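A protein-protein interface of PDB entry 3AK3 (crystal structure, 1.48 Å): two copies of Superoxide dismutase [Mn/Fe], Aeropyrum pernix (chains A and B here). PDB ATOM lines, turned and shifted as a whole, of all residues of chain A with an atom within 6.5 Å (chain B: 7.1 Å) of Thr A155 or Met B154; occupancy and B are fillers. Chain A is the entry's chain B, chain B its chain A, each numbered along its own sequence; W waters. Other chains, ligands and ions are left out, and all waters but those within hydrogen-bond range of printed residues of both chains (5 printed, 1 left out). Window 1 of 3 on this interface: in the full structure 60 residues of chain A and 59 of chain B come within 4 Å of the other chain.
The side-chain hydroxyl of Ser B70 lies within hydrogen-bond range of the backbone carbonyl oxygen of Leu A153 (2.6 Å). The backbone carbonyl oxygen of Asn B151 lies within hydrogen-bond range of the backbone NH of Leu A153. O of Leu B153 sits at hydrogen-bond distance from OG of Ser A70, at 2.6 Å. The backbone carbonyl oxygen of Asn A151 lies within hydrogen-bond range of the backbone NH of Leu B153 (2.7 Å).
The side-chain hydroxyl (OG) of Ser B70 sits at hydrogen-bond distance from the side-chain amide nitrogen (ND2) of Asn B151. N of Phe B71 lies close to ND2 of Asn B151 (3.4 Å). OG of Ser A70 lies within hydrogen-bond range of ND2 of Asn A151. The backbone NH of Gly A157 sits at hydrogen-bond distance from the side-chain hydroxyl of Tyr A210.
Among the printed residues, pairs that only touch across the chains: Ser A70 with Thr B155, Ala A74 with Thr B155, Asn A151 with Val B152, Asn A151 with Met B154, Val A152 with Asn B151, Met A154 with Asn B151, Met A154 with Met B154, Met A154 with Thr B155, Met A154 with Ala B156, Thr A155 with Ser B70, Thr A155 with Tyr B73, Thr A155 with Ala B74, Thr A155 with Met B154, Ala A156 with Tyr B73, Ala A156 with Ile B77, Ala A156 with Met B78, Ala A156 with Met B154, Ala A156 with Pro B160, Gly A157 with Ile B77, Leu A158 with Tyr B73, Tyr A210 with Val B159 and Tyr A210 with Pro B160.
Met B154 touches four residues of chain A. Printed residues of chain A within 4 Å of Met B78: Ala A156. Printed residues of chain B within 4 Å of Ala A156: Tyr B73, Ile B77, Met B78, Met B154 and Pro B160. Of the printed residues of chain A, Leu B153 touches Ser A70 and Asn A151. Printed residues of chain A within 4 Å of Ala B74: Thr A155. The nearest printed residue of chain B that does not touch Thr A155 is Asn B151 (4.4 Å). The nearest residue of chain A that does not touch Met B154 is Ser A70 (4.6 Å).
Printed residues of chain A that touch a printed residue of chain B: Ser A70, Ala A74, Asn A151, Val A152, Leu A153, Met A154, Thr A155, Ala A156, Gly A157, Leu A158 and Tyr A210. Hydrophobic or aromatic side chains of chain A within 4 Å of the printed part of chain B: Ala A74, Leu A153, Met A154, Ala A156, Leu A158 and Tyr A210. Of the 26 printed residues of chain B, 13 touch a printed residue of chain A. Along chain B the printed residues that touch a printed residue of chain A span positions 70 to 160. Among the printed residues, 26 pairs touch across the chains. Among the printed residues, no Asp or Glu carboxylate lies within 4 Å of a Lys or Arg side-chain nitrogen of the other chain.
Asn A151 touches Met B154, and with the chains exchanged Met A154 touches Asn B151. Met A154 touches Thr B155, and with the chains exchanged Thr A155 touches Met B154. Met A154 touches Ala B156, and with the chains exchanged Ala A156 touches Met B154. Of the 26 pairs that touch across the chains among the printed residues, 17 have their exchanged pair printed and touching as well.
Water W5 lies within hydrogen-bond range of the backbone carbonyl oxygen of Leu B158 (2.6 Å), the backbone NH of Gly A157 (2.9 Å) and the side-chain hydroxyl of Tyr A210 (2.9 Å). Water W2 lies within hydrogen-bond range of the backbone carbonyl oxygen (O) of His B150 (2.8 Å), the backbone NH (N) of Ala A156 (2.9 Å) and the side-chain sulfur (SD) of Met B78 (3.4 Å).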
ATOM      1  N   SER A  70      11.732  -3.694   0.207  1.00  0.00           N
ATOM      2  CA  SER A  70      10.528  -4.096  -0.540  1.00  0.00           C
ATOM      3  C   SER A  70       9.517  -4.833   0.332  1.00  0.00           C
ATOM      4  O   SER A  70       8.372  -4.431   0.393  1.00  0.00           O
ATOM      5  CB  SER A  70      10.906  -4.938  -1.774  1.00  0.00           C
ATOM      6  OG  SER A  70       9.772  -5.619  -2.323  1.00  0.00           O
ATOM      7  N   ALA A  74       6.216  -2.901   1.713  1.00  0.00           N
ATOM      8  CA  ALA A  74       4.967  -3.494   1.246  1.00  0.00           C
ATOM      9  C   ALA A  74       4.099  -3.919   2.429  1.00  0.00           C
ATOM     10  O   ALA A  74       2.905  -3.636   2.441  1.00  0.00           O
ATOM     11  CB  ALA A  74       5.245  -4.668   0.344  1.00  0.00           C
ATOM     12  N   LEU A 145      -6.728  -9.121  -7.983  1.00  0.00           N
ATOM     13  CA  LEU A 145      -5.529  -9.967  -8.058  1.00  0.00           C
ATOM     14  C   LEU A 145      -5.152 -10.504  -6.687  1.00  0.00           C
ATOM     15  O   LEU A 145      -5.719 -10.083  -5.663  1.00  0.00           O
ATOM     16  CB  LEU A 145      -4.343  -9.221  -8.705  1.00  0.00           C
ATOM     17  CG  LEU A 145      -3.599  -8.123  -7.923  1.00  0.00           C
ATOM     18  CD1 LEU A 145      -2.193  -7.835  -8.508  1.00  0.00           C
ATOM     19  CD2 LEU A 145      -4.445  -6.851  -7.893  1.00  0.00           C
ATOM     20  N   VAL A 147      -1.780 -11.121  -4.077  1.00  0.00           N
ATOM     21  CA  VAL A 147      -0.384 -10.816  -3.771  1.00  0.00           C
ATOM     22  C   VAL A 147       0.092 -11.899  -2.826  1.00  0.00           C
ATOM     23  O   VAL A 147      -0.624 -12.262  -1.877  1.00  0.00           O
ATOM     24  CB  VAL A 147      -0.251  -9.403  -3.133  1.00  0.00           C
ATOM     25  CG1 VAL A 147       1.162  -9.118  -2.600  1.00  0.00           C
ATOM     26  CG2 VAL A 147      -0.687  -8.349  -4.112  1.00  0.00           C
ATOM     27  N   HIS A 150       4.093  -9.970   0.817  1.00  0.00           N
ATOM     28  CA  HIS A 150       3.572  -8.608   0.627  1.00  0.00           C
ATOM     29  C   HIS A 150       3.935  -8.000  -0.703  1.00  0.00           C
ATOM     30  O   HIS A 150       3.408  -6.960  -1.085  1.00  0.00           O
ATOM     31  CB  HIS A 150       4.080  -7.688   1.726  1.00  0.00           C
ATOM     32  CG  HIS A 150       3.650  -8.119   3.080  1.00  0.00           C
ATOM     33  ND1 HIS A 150       4.508  -8.245   4.148  1.00  0.00           N
ATOM     34  CD2 HIS A 150       2.435  -8.520   3.521  1.00  0.00           C
ATOM     35  CE1 HIS A 150       3.832  -8.679   5.197  1.00  0.00           C
ATOM     36  NE2 HIS A 150       2.574  -8.851   4.842  1.00  0.00           N
ATOM     37  N   ASN A 151       4.847  -8.674  -1.402  1.00  0.00           N
ATOM     38  CA  ASN A 151       5.582  -8.030  -2.489  1.00  0.00           C
ATOM     39  C   ASN A 151       5.874  -9.002  -3.606  1.00  0.00           C
ATOM     40  O   ASN A 151       6.917  -8.920  -4.254  1.00  0.00           O
ATOM     41  CB  ASN A 151       6.889  -7.432  -1.948  1.00  0.00           C
ATOM     42  CG  ASN A 151       7.846  -8.498  -1.405  1.00  0.00           C
ATOM     43  OD1 ASN A 151       7.433  -9.590  -1.008  1.00  0.00           O
ATOM     44  ND2 ASN A 151       9.138  -8.170  -1.370  1.00  0.00           N
ATOM     45  N   VAL A 152       4.967  -9.951  -3.830  1.00  0.00           N
ATOM     46  CA  VAL A 152       5.101 -10.885  -4.947  1.00  0.00           C
ATOM     47  C   VAL A 152       3.767 -10.875  -5.675  1.00  0.00           C
ATOM     48  O   VAL A 152       2.727 -10.999  -5.037  1.00  0.00           O
ATOM     49  CB  VAL A 152       5.459 -12.312  -4.482  1.00  0.00           C
ATOM     50  CG1 VAL A 152       5.536 -13.270  -5.681  1.00  0.00           C
ATOM     51  CG2 VAL A 152       6.773 -12.321  -3.716  1.00  0.00           C
ATOM     52  N   LEU A 153       3.794 -10.748  -6.997  1.00  0.00           N
ATOM     53  CA  LEU A 153       2.582 -10.629  -7.838  1.00  0.00           C
ATOM     54  C   LEU A 153       1.984  -9.235  -7.838  1.00  0.00           C
ATOM     55  O   LEU A 153       1.204  -8.909  -8.719  1.00  0.00           O
ATOM     56  CB  LEU A 153       1.502 -11.655  -7.499  1.00  0.00           C
ATOM     57  CG  LEU A 153       1.948 -13.108  -7.516  1.00  0.00           C
ATOM     58  CD1 LEU A 153       0.727 -13.965  -7.226  1.00  0.00           C
ATOM     59  CD2 LEU A 153       2.581 -13.505  -8.842  1.00  0.00           C
ATOM     60  N   MET A 154       2.385  -8.388  -6.891  1.00  0.00           N
ATOM     61  CA  MET A 154       1.992  -6.990  -7.020  1.00  0.00           C
ATOM     62  C   MET A 154       2.658  -6.326  -8.219  1.00  0.00           C
ATOM     63  O   MET A 154       3.812  -6.644  -8.578  1.00  0.00           O
ATOM     64  CB  MET A 154       2.279  -6.191  -5.754  1.00  0.00           C
ATOM     65  CG  MET A 154       1.652  -4.791  -5.794  1.00  0.00           C
ATOM     66  SD  MET A 154      -0.148  -4.828  -6.112  1.00  0.00           S
ATOM     67  CE  MET A 154      -0.552  -3.089  -6.292  1.00  0.00           C
ATOM     68  N   THR A 155       1.930  -5.417  -8.853  1.00  0.00           N
ATOM     69  CA  THR A 155       2.446  -4.749 -10.045  1.00  0.00           C
ATOM     70  C   THR A 155       2.511  -3.247  -9.812  1.00  0.00           C
ATOM     71  O   THR A 155       1.860  -2.726  -8.912  1.00  0.00           O
ATOM     72  CB  THR A 155       1.559  -5.011 -11.289  1.00  0.00           C
ATOM     73  OG1 THR A 155       0.348  -4.248 -11.198  1.00  0.00           O
ATOM     74  CG2 THR A 155       1.192  -6.499 -11.421  1.00  0.00           C
ATOM     75  N   ALA A 156       3.261  -2.541 -10.651  1.00  0.00           N
ATOM     76  CA  ALA A 156       3.146  -1.083 -10.706  1.00  0.00           C
ATOM     77  C   ALA A 156       1.758  -0.665 -11.185  1.00  0.00           C
ATOM     78  O   ALA A 156       1.011  -1.477 -11.743  1.00  0.00           O
ATOM     79  CB  ALA A 156       4.222  -0.514 -11.640  1.00  0.00           C
ATOM     80  N   GLY A 157       1.407   0.598 -10.945  1.00  0.00           N
ATOM     81  CA  GLY A 157       0.163   1.175 -11.453  1.00  0.00           C
ATOM     82  C   GLY A 157      -1.069   0.915 -10.609  1.00  0.00           C
ATOM     83  O   GLY A 157      -1.688   1.860 -10.093  1.00  0.00           O
ATOM     84  N   LEU A 158      -1.453  -0.358 -10.503  1.00  0.00           N
ATOM     85  CA  LEU A 158      -2.655  -0.768  -9.773  1.00  0.00           C
ATOM     86  C   LEU A 158      -2.676  -0.162  -8.389  1.00  0.00           C
ATOM     87  O   LEU A 158      -1.710  -0.266  -7.652  1.00  0.00           O
ATOM     88  CB  LEU A 158      -2.732  -2.295  -9.658  1.00  0.00           C
ATOM     89  CG  LEU A 158      -2.760  -3.043 -10.991  1.00  0.00           C
ATOM     90  CD1 LEU A 158      -2.816  -4.565 -10.776  1.00  0.00           C
ATOM     91  CD2 LEU A 158      -3.915  -2.569 -11.893  1.00  0.00           C
ATOM     92  N   TYR A 210       0.815   8.062 -14.889  1.00  0.00           N
ATOM     93  CA  TYR A 210       1.362   7.099 -15.839  1.00  0.00           C
ATOM     94  C   TYR A 210       1.170   7.517 -17.279  1.00  0.00           C
ATOM     95  O   TYR A 210       2.066   7.342 -18.118  1.00  0.00           O
ATOM     96  CB  TYR A 210       0.716   5.740 -15.599  1.00  0.00           C
ATOM     97  CG  TYR A 210       1.030   5.247 -14.223  1.00  0.00           C
ATOM     98  CD1 TYR A 210       2.314   4.802 -13.914  1.00  0.00           C
ATOM     99  CD2 TYR A 210       0.067   5.275 -13.209  1.00  0.00           C
ATOM    100  CE1 TYR A 210       2.632   4.369 -12.653  1.00  0.00           C
ATOM    101  CE2 TYR A 210       0.379   4.840 -11.935  1.00  0.00           C
ATOM    102  CZ  TYR A 210       1.670   4.389 -11.666  1.00  0.00           C
ATOM    103  OH  TYR A 210       2.020   3.942 -10.418  1.00  0.00           O
ATOM    104  N   PHE B  69      -2.467 -12.479 -15.371  1.00  0.00           N
ATOM    105  CA  PHE B  69      -2.777 -11.073 -15.448  1.00  0.00           C
ATOM    106  C   PHE B  69      -1.681 -10.223 -14.811  1.00  0.00           C
ATOM    107  O   PHE B  69      -1.249  -9.219 -15.386  1.00  0.00           O
ATOM    108  CB  PHE B  69      -4.108 -10.757 -14.771  1.00  0.00           C
ATOM    109  CG  PHE B  69      -4.373  -9.284 -14.686  1.00  0.00           C
ATOM    110  CD1 PHE B  69      -4.156  -8.587 -13.497  1.00  0.00           C
ATOM    111  CD2 PHE B  69      -4.727  -8.587 -15.830  1.00  0.00           C
ATOM    112  CE1 PHE B  69      -4.369  -7.198 -13.467  1.00  0.00           C
ATOM    113  CE2 PHE B  69      -4.928  -7.209 -15.787  1.00  0.00           C
ATOM    114  CZ  PHE B  69      -4.754  -6.538 -14.610  1.00  0.00           C
ATOM    115  N   SER B  70      -1.255 -10.631 -13.621  1.00  0.00           N
ATOM    116  CA  SER B  70      -0.223  -9.895 -12.899  1.00  0.00           C
ATOM    117  C   SER B  70       1.017  -9.737 -13.746  1.00  0.00           C
ATOM    118  O   SER B  70       1.505  -8.636 -13.953  1.00  0.00           O
ATOM    119  CB  SER B  70       0.146 -10.611 -11.605  1.00  0.00           C
ATOM    120  OG  SER B  70       1.337 -10.079 -11.019  1.00  0.00           O
ATOM    121  N   PHE B  71       1.527 -10.857 -14.239  1.00  0.00           N
ATOM    122  CA  PHE B  71       2.771 -10.814 -15.000  1.00  0.00           C
ATOM    123  C   PHE B  71       2.647  -9.962 -16.256  1.00  0.00           C
ATOM    124  O   PHE B  71       3.507  -9.116 -16.530  1.00  0.00           O
ATOM    125  CB  PHE B  71       3.241 -12.217 -15.361  1.00  0.00           C
ATOM    126  CG  PHE B  71       4.448 -12.236 -16.279  1.00  0.00           C
ATOM    127  CD1 PHE B  71       5.726 -12.119 -15.757  1.00  0.00           C
ATOM    128  CD2 PHE B  71       4.295 -12.387 -17.649  1.00  0.00           C
ATOM    129  CE1 PHE B  71       6.843 -12.122 -16.595  1.00  0.00           C
ATOM    130  CE2 PHE B  71       5.413 -12.404 -18.501  1.00  0.00           C
ATOM    131  CZ  PHE B  71       6.677 -12.264 -17.965  1.00  0.00           C
ATOM    132  N   ASN B  72       1.585 -10.175 -17.031  1.00  0.00           N
ATOM    133  CA  ASN B  72       1.434  -9.463 -18.305  1.00  0.00           C
ATOM    134  C   ASN B  72       1.052  -7.992 -18.143  1.00  0.00           C
ATOM    135  O   ASN B  72       1.596  -7.124 -18.825  1.00  0.00           O
ATOM    136  CB  ASN B  72       0.505 -10.220 -19.249  1.00  0.00           C
ATOM    137  CG  ASN B  72       1.137 -11.493 -19.734  1.00  0.00           C
ATOM    138  OD1 ASN B  72       2.066 -11.465 -20.543  1.00  0.00           O
ATOM    139  ND2 ASN B  72       0.702 -12.619 -19.182  1.00  0.00           N
ATOM    140  N   TYR B  73       0.141  -7.704 -17.224  1.00  0.00           N
ATOM    141  CA  TYR B  73      -0.159  -6.313 -16.929  1.00  0.00           C
ATOM    142  C   TYR B  73       1.114  -5.583 -16.491  1.00  0.00           C
ATOM    143  O   TYR B  73       1.387  -4.456 -16.944  1.00  0.00           O
ATOM    144  CB  TYR B  73      -1.203  -6.200 -15.820  1.00  0.00           C
ATOM    145  CG  TYR B  73      -1.483  -4.759 -15.481  1.00  0.00           C
ATOM    146  CD1 TYR B  73      -2.426  -4.021 -16.200  1.00  0.00           C
ATOM    147  CD2 TYR B  73      -0.756  -4.110 -14.479  1.00  0.00           C
ATOM    148  CE1 TYR B  73      -2.658  -2.663 -15.909  1.00  0.00           C
ATOM    149  CE2 TYR B  73      -0.979  -2.763 -14.190  1.00  0.00           C
ATOM    150  CZ  TYR B  73      -1.943  -2.054 -14.904  1.00  0.00           C
ATOM    151  OH  TYR B  73      -2.166  -0.724 -14.615  1.00  0.00           O
ATOM    152  N   ALA B  74       1.868  -6.213 -15.595  1.00  0.00           N
ATOM    153  CA  ALA B  74       3.113  -5.610 -15.104  1.00  0.00           C
ATOM    154  C   ALA B  74       4.087  -5.369 -16.249  1.00  0.00           C
ATOM    155  O   ALA B  74       4.682  -4.295 -16.353  1.00  0.00           O
ATOM    156  CB  ALA B  74       3.730  -6.460 -14.066  1.00  0.00           C
ATOM    157  N   GLY B  75       4.262  -6.369 -17.113  1.00  0.00           N
ATOM    158  CA  GLY B  75       5.123  -6.173 -18.293  1.00  0.00           C
ATOM    159  C   GLY B  75       4.641  -4.985 -19.125  1.00  0.00           C
ATOM    160  O   GLY B  75       5.425  -4.160 -19.617  1.00  0.00           O
ATOM    161  N   ILE B  77       2.691  -2.211 -18.240  1.00  0.00           N
ATOM    162  CA  ILE B  77       2.873  -0.896 -17.640  1.00  0.00           C
ATOM    163  C   ILE B  77       4.355  -0.542 -17.523  1.00  0.00           C
ATOM    164  O   ILE B  77       4.743   0.607 -17.754  1.00  0.00           O
ATOM    165  CB  ILE B  77       2.135  -0.738 -16.294  1.00  0.00           C
ATOM    166  CG1 ILE B  77       2.026   0.750 -15.943  1.00  0.00           C
ATOM    167  CG2 ILE B  77       2.804  -1.536 -15.166  1.00  0.00           C
ATOM    168  CD1 ILE B  77       1.088   1.047 -14.797  1.00  0.00           C
ATOM    169  N   MET B  78       5.192  -1.531 -17.209  1.00  0.00           N
ATOM    170  CA  MET B  78       6.620  -1.231 -17.038  1.00  0.00           C
ATOM    171  C   MET B  78       7.242  -0.784 -18.362  1.00  0.00           C
ATOM    172  O   MET B  78       8.004   0.173 -18.377  1.00  0.00           O
ATOM    173  CB  MET B  78       7.391  -2.414 -16.446  1.00  0.00           C
ATOM    174  CG  MET B  78       6.992  -2.823 -15.035  1.00  0.00           C
ATOM    175  SD  MET B  78       7.325  -1.563 -13.778  1.00  0.00           S
ATOM    176  CE  MET B  78       9.119  -1.688 -13.622  1.00  0.00           C
ATOM    177  N   VAL B 132      14.449   0.416 -10.550  1.00  0.00           N
ATOM    178  CA  VAL B 132      13.329   1.349 -10.433  1.00  0.00           C
ATOM    179  C   VAL B 132      13.616   2.532  -9.500  1.00  0.00           C
ATOM    180  O   VAL B 132      14.007   2.351  -8.348  1.00  0.00           O
ATOM    181  CB  VAL B 132      12.022   0.611  -9.969  1.00  0.00           C
ATOM    182  CG1 VAL B 132      10.845   1.606  -9.786  1.00  0.00           C
ATOM    183  CG2 VAL B 132      11.634  -0.506 -10.940  1.00  0.00           C
ATOM    184  N   ALA B 134      11.313   5.226  -7.820  1.00  0.00           N
ATOM    185  CA  ALA B 134       9.912   5.421  -7.514  1.00  0.00           C
ATOM    186  C   ALA B 134       9.687   6.615  -6.612  1.00  0.00           C
ATOM    187  O   ALA B 134      10.564   6.980  -5.837  1.00  0.00           O
ATOM    188  CB  ALA B 134       9.339   4.173  -6.856  1.00  0.00           C
ATOM    189  N   LEU B 145      14.483   0.769  -5.875  1.00  0.00           N
ATOM    190  CA  LEU B 145      14.276  -0.659  -5.662  1.00  0.00           C
ATOM    191  C   LEU B 145      14.520  -1.468  -6.931  1.00  0.00           C
ATOM    192  O   LEU B 145      14.649  -0.914  -8.015  1.00  0.00           O
ATOM    193  CB  LEU B 145      12.875  -0.943  -5.074  1.00  0.00           C
ATOM    194  CG  LEU B 145      11.602  -0.876  -5.930  1.00  0.00           C
ATOM    195  CD1 LEU B 145      10.495  -1.642  -5.224  1.00  0.00           C
ATOM    196  CD2 LEU B 145      11.163   0.560  -6.153  1.00  0.00           C
ATOM    197  N   GLN B 146      14.572  -2.785  -6.771  1.00  0.00           N
ATOM    198  CA  GLN B 146      14.586  -3.715  -7.883  1.00  0.00           C
ATOM    199  C   GLN B 146      13.234  -4.385  -8.010  1.00  0.00           C
ATOM    200  O   GLN B 146      12.513  -4.586  -7.015  1.00  0.00           O
ATOM    201  CB  GLN B 146      15.594  -4.830  -7.639  1.00  0.00           C
ATOM    202  CG  GLN B 146      17.036  -4.379  -7.477  1.00  0.00           C
ATOM    203  CD  GLN B 146      17.956  -5.549  -7.172  1.00  0.00           C
ATOM    204  OE1 GLN B 146      17.548  -6.517  -6.541  1.00  0.00           O
ATOM    205  NE2 GLN B 146      19.217  -5.458  -7.608  1.00  0.00           N
ATOM    206  N   VAL B 147      12.933  -4.788  -9.227  1.00  0.00           N
ATOM    207  CA  VAL B 147      11.815  -5.673  -9.507  1.00  0.00           C
ATOM    208  C   VAL B 147      12.361  -6.861 -10.291  1.00  0.00           C
ATOM    209  O   VAL B 147      13.151  -6.671 -11.220  1.00  0.00           O
ATOM    210  CB  VAL B 147      10.732  -4.948 -10.312  1.00  0.00           C
ATOM    211  CG1 VAL B 147       9.668  -5.932 -10.811  1.00  0.00           C
ATOM    212  CG2 VAL B 147      10.106  -3.821  -9.478  1.00  0.00           C
ATOM    213  N   GLU B 148      11.983  -8.073  -9.886  1.00  0.00           N
ATOM    214  CA  GLU B 148      12.343  -9.299 -10.605  1.00  0.00           C
ATOM    215  C   GLU B 148      11.181  -9.687 -11.497  1.00  0.00           C
ATOM    216  O   GLU B 148      10.041  -9.407 -11.167  1.00  0.00           O
ATOM    217  CB  GLU B 148      12.699 -10.438  -9.638  1.00  0.00           C
ATOM    218  CG  GLU B 148      14.057 -10.244  -8.953  1.00  0.00           C
ATOM    219  CD  GLU B 148      14.434 -11.341  -7.949  1.00  0.00           C
ATOM    220  OE1 GLU B 148      15.280 -11.045  -7.067  1.00  0.00           O
ATOM    221  OE2 GLU B 148      13.908 -12.481  -8.051  1.00  0.00           O
ATOM    222  N   HIS B 150       8.504  -9.017 -13.839  1.00  0.00           N
ATOM    223  CA  HIS B 150       7.811  -7.730 -13.918  1.00  0.00           C
ATOM    224  C   HIS B 150       7.033  -7.458 -12.655  1.00  0.00           C
ATOM    225  O   HIS B 150       6.553  -6.333 -12.457  1.00  0.00           O
ATOM    226  CB  HIS B 150       6.852  -7.738 -15.100  1.00  0.00           C
ATOM    227  CG  HIS B 150       7.553  -7.840 -16.413  1.00  0.00           C
ATOM    228  ND1 HIS B 150       7.140  -8.668 -17.434  1.00  0.00           N
ATOM    229  CD2 HIS B 150       8.663  -7.211 -16.858  1.00  0.00           C
ATOM    230  CE1 HIS B 150       7.975  -8.542 -18.453  1.00  0.00           C
ATOM    231  NE2 HIS B 150       8.900  -7.659 -18.130  1.00  0.00           N
ATOM    232  N   ASN B 151       6.915  -8.487 -11.811  1.00  0.00           N
ATOM    233  CA  ASN B 151       5.863  -8.531 -10.780  1.00  0.00           C
ATOM    234  C   ASN B 151       6.337  -9.266  -9.537  1.00  0.00           C
ATOM    235  O   ASN B 151       5.553  -9.946  -8.871  1.00  0.00           O
ATOM    236  CB  ASN B 151       4.606  -9.222 -11.332  1.00  0.00           C
ATOM    237  CG  ASN B 151       4.857 -10.675 -11.703  1.00  0.00           C
ATOM    238  OD1 ASN B 151       5.990 -11.083 -11.994  1.00  0.00           O
ATOM    239  ND2 ASN B 151       3.801 -11.461 -11.720  1.00  0.00           N
ATOM    240  N   VAL B 152       7.624  -9.138  -9.220  1.00  0.00           N
ATOM    241  CA  VAL B 152       8.171  -9.704  -8.009  1.00  0.00           C
ATOM    242  C   VAL B 152       9.026  -8.612  -7.361  1.00  0.00           C
ATOM    243  O   VAL B 152       9.845  -7.980  -8.038  1.00  0.00           O
ATOM    244  CB  VAL B 152       9.017 -10.982  -8.291  1.00  0.00           C
ATOM    245  CG1 VAL B 152       9.595 -11.550  -6.998  1.00  0.00           C
ATOM    246  CG2 VAL B 152       8.196 -12.050  -9.053  1.00  0.00           C
ATOM    247  N   LEU B 153       8.825  -8.371  -6.071  1.00  0.00           N
ATOM    248  CA  LEU B 153       9.484  -7.278  -5.321  1.00  0.00           C
ATOM    249  C   LEU B 153       8.855  -5.919  -5.529  1.00  0.00           C
ATOM    250  O   LEU B 153       9.131  -5.015  -4.750  1.00  0.00           O
ATOM    251  CB  LEU B 153      11.000  -7.145  -5.578  1.00  0.00           C
ATOM    252  CG  LEU B 153      11.832  -8.408  -5.462  1.00  0.00           C
ATOM    253  CD1 LEU B 153      13.284  -8.042  -5.668  1.00  0.00           C
ATOM    254  CD2 LEU B 153      11.672  -9.080  -4.123  1.00  0.00           C
ATOM    255  N   MET B 154       8.041  -5.730  -6.564  1.00  0.00           N
ATOM    256  CA  MET B 154       7.240  -4.500  -6.629  1.00  0.00           C
ATOM    257  C   MET B 154       6.252  -4.491  -5.470  1.00  0.00           C
ATOM    258  O   MET B 154       5.775  -5.537  -5.024  1.00  0.00           O
ATOM    259  CB  MET B 154       6.512  -4.376  -7.970  1.00  0.00           C
ATOM    260  CG  MET B 154       5.855  -3.027  -8.204  1.00  0.00           C
ATOM    261  SD  MET B 154       7.049  -1.702  -7.962  1.00  0.00           S
ATOM    262  CE  MET B 154       5.959  -0.291  -8.120  1.00  0.00           C
ATOM    263  N   THR B 155       5.981  -3.286  -4.979  1.00  0.00           N
ATOM    264  CA  THR B 155       5.056  -3.084  -3.872  1.00  0.00           C
ATOM    265  C   THR B 155       3.920  -2.178  -4.322  1.00  0.00           C
ATOM    266  O   THR B 155       4.027  -1.453  -5.306  1.00  0.00           O
ATOM    267  CB  THR B 155       5.761  -2.420  -2.679  1.00  0.00           C
ATOM    268  OG1 THR B 155       5.951  -1.034  -2.951  1.00  0.00           O
ATOM    269  CG2 THR B 155       7.121  -3.053  -2.420  1.00  0.00           C
ATOM    270  N   ALA B 156       2.826  -2.202  -3.569  1.00  0.00           N
ATOM    271  CA  ALA B 156       1.837  -1.147  -3.698  1.00  0.00           C
ATOM    272  C   ALA B 156       2.422   0.238  -3.358  1.00  0.00           C
ATOM    273  O   ALA B 156       3.472   0.358  -2.708  1.00  0.00           O
ATOM    274  CB  ALA B 156       0.670  -1.438  -2.774  1.00  0.00           C
ATOM    275  N   GLY B 157       1.719   1.277  -3.791  1.00  0.00           N
ATOM    276  CA  GLY B 157       2.052   2.647  -3.411  1.00  0.00           C
ATOM    277  C   GLY B 157       3.087   3.303  -4.294  1.00  0.00           C
ATOM    278  O   GLY B 157       2.781   4.250  -5.018  1.00  0.00           O
ATOM    279  N   LEU B 158       4.310   2.773  -4.243  1.00  0.00           N
ATOM    280  CA  LEU B 158       5.425   3.326  -5.007  1.00  0.00           C
ATOM    281  C   LEU B 158       5.081   3.522  -6.470  1.00  0.00           C
ATOM    282  O   LEU B 158       4.585   2.602  -7.131  1.00  0.00           O
ATOM    283  CB  LEU B 158       6.687   2.458  -4.880  1.00  0.00           C
ATOM    284  CG  LEU B 158       7.205   2.099  -3.485  1.00  0.00           C
ATOM    285  CD1 LEU B 158       8.414   1.166  -3.524  1.00  0.00           C
ATOM    286  CD2 LEU B 158       7.496   3.344  -2.641  1.00  0.00           C
ATOM    287  N   VAL B 159       5.370   4.720  -6.967  1.00  0.00           N
ATOM    288  CA  VAL B 159       5.104   5.093  -8.351  1.00  0.00           C
ATOM    289  C   VAL B 159       6.415   5.131  -9.128  1.00  0.00           C
ATOM    290  O   VAL B 159       7.216   6.032  -8.893  1.00  0.00           O
ATOM    291  CB  VAL B 159       4.449   6.494  -8.411  1.00  0.00           C
ATOM    292  CG1 VAL B 159       4.152   6.921  -9.856  1.00  0.00           C
ATOM    293  CG2 VAL B 159       3.195   6.529  -7.541  1.00  0.00           C
ATOM    294  N   PRO B 160       6.650   4.171 -10.049  1.00  0.00           N
ATOM    295  CA  PRO B 160       7.891   4.272 -10.827  1.00  0.00           C
ATOM    296  C   PRO B 160       7.883   5.526 -11.688  1.00  0.00           C
ATOM    297  O   PRO B 160       6.921   5.786 -12.407  1.00  0.00           O
ATOM    298  CB  PRO B 160       7.852   3.024 -11.717  1.00  0.00           C
ATOM    299  CG  PRO B 160       6.935   2.081 -10.992  1.00  0.00           C
ATOM    300  CD  PRO B 160       5.865   2.990 -10.445  1.00  0.00           C
HETATM  301  O   HOH W   1       0.328   0.776  -6.304  1.00  0.00           O
HETATM  302  O   HOH W   2       5.517  -3.762 -11.980  1.00  0.00           O
HETATM  303  O   HOH W   3       2.219  -4.520  -1.977  1.00  0.00           O
HETATM  304  O   HOH W   4       2.228  -0.702  -7.251  1.00  0.00           O
HETATM  305  O   HOH W   5       2.592   1.719  -8.571  1.00  0.00           O
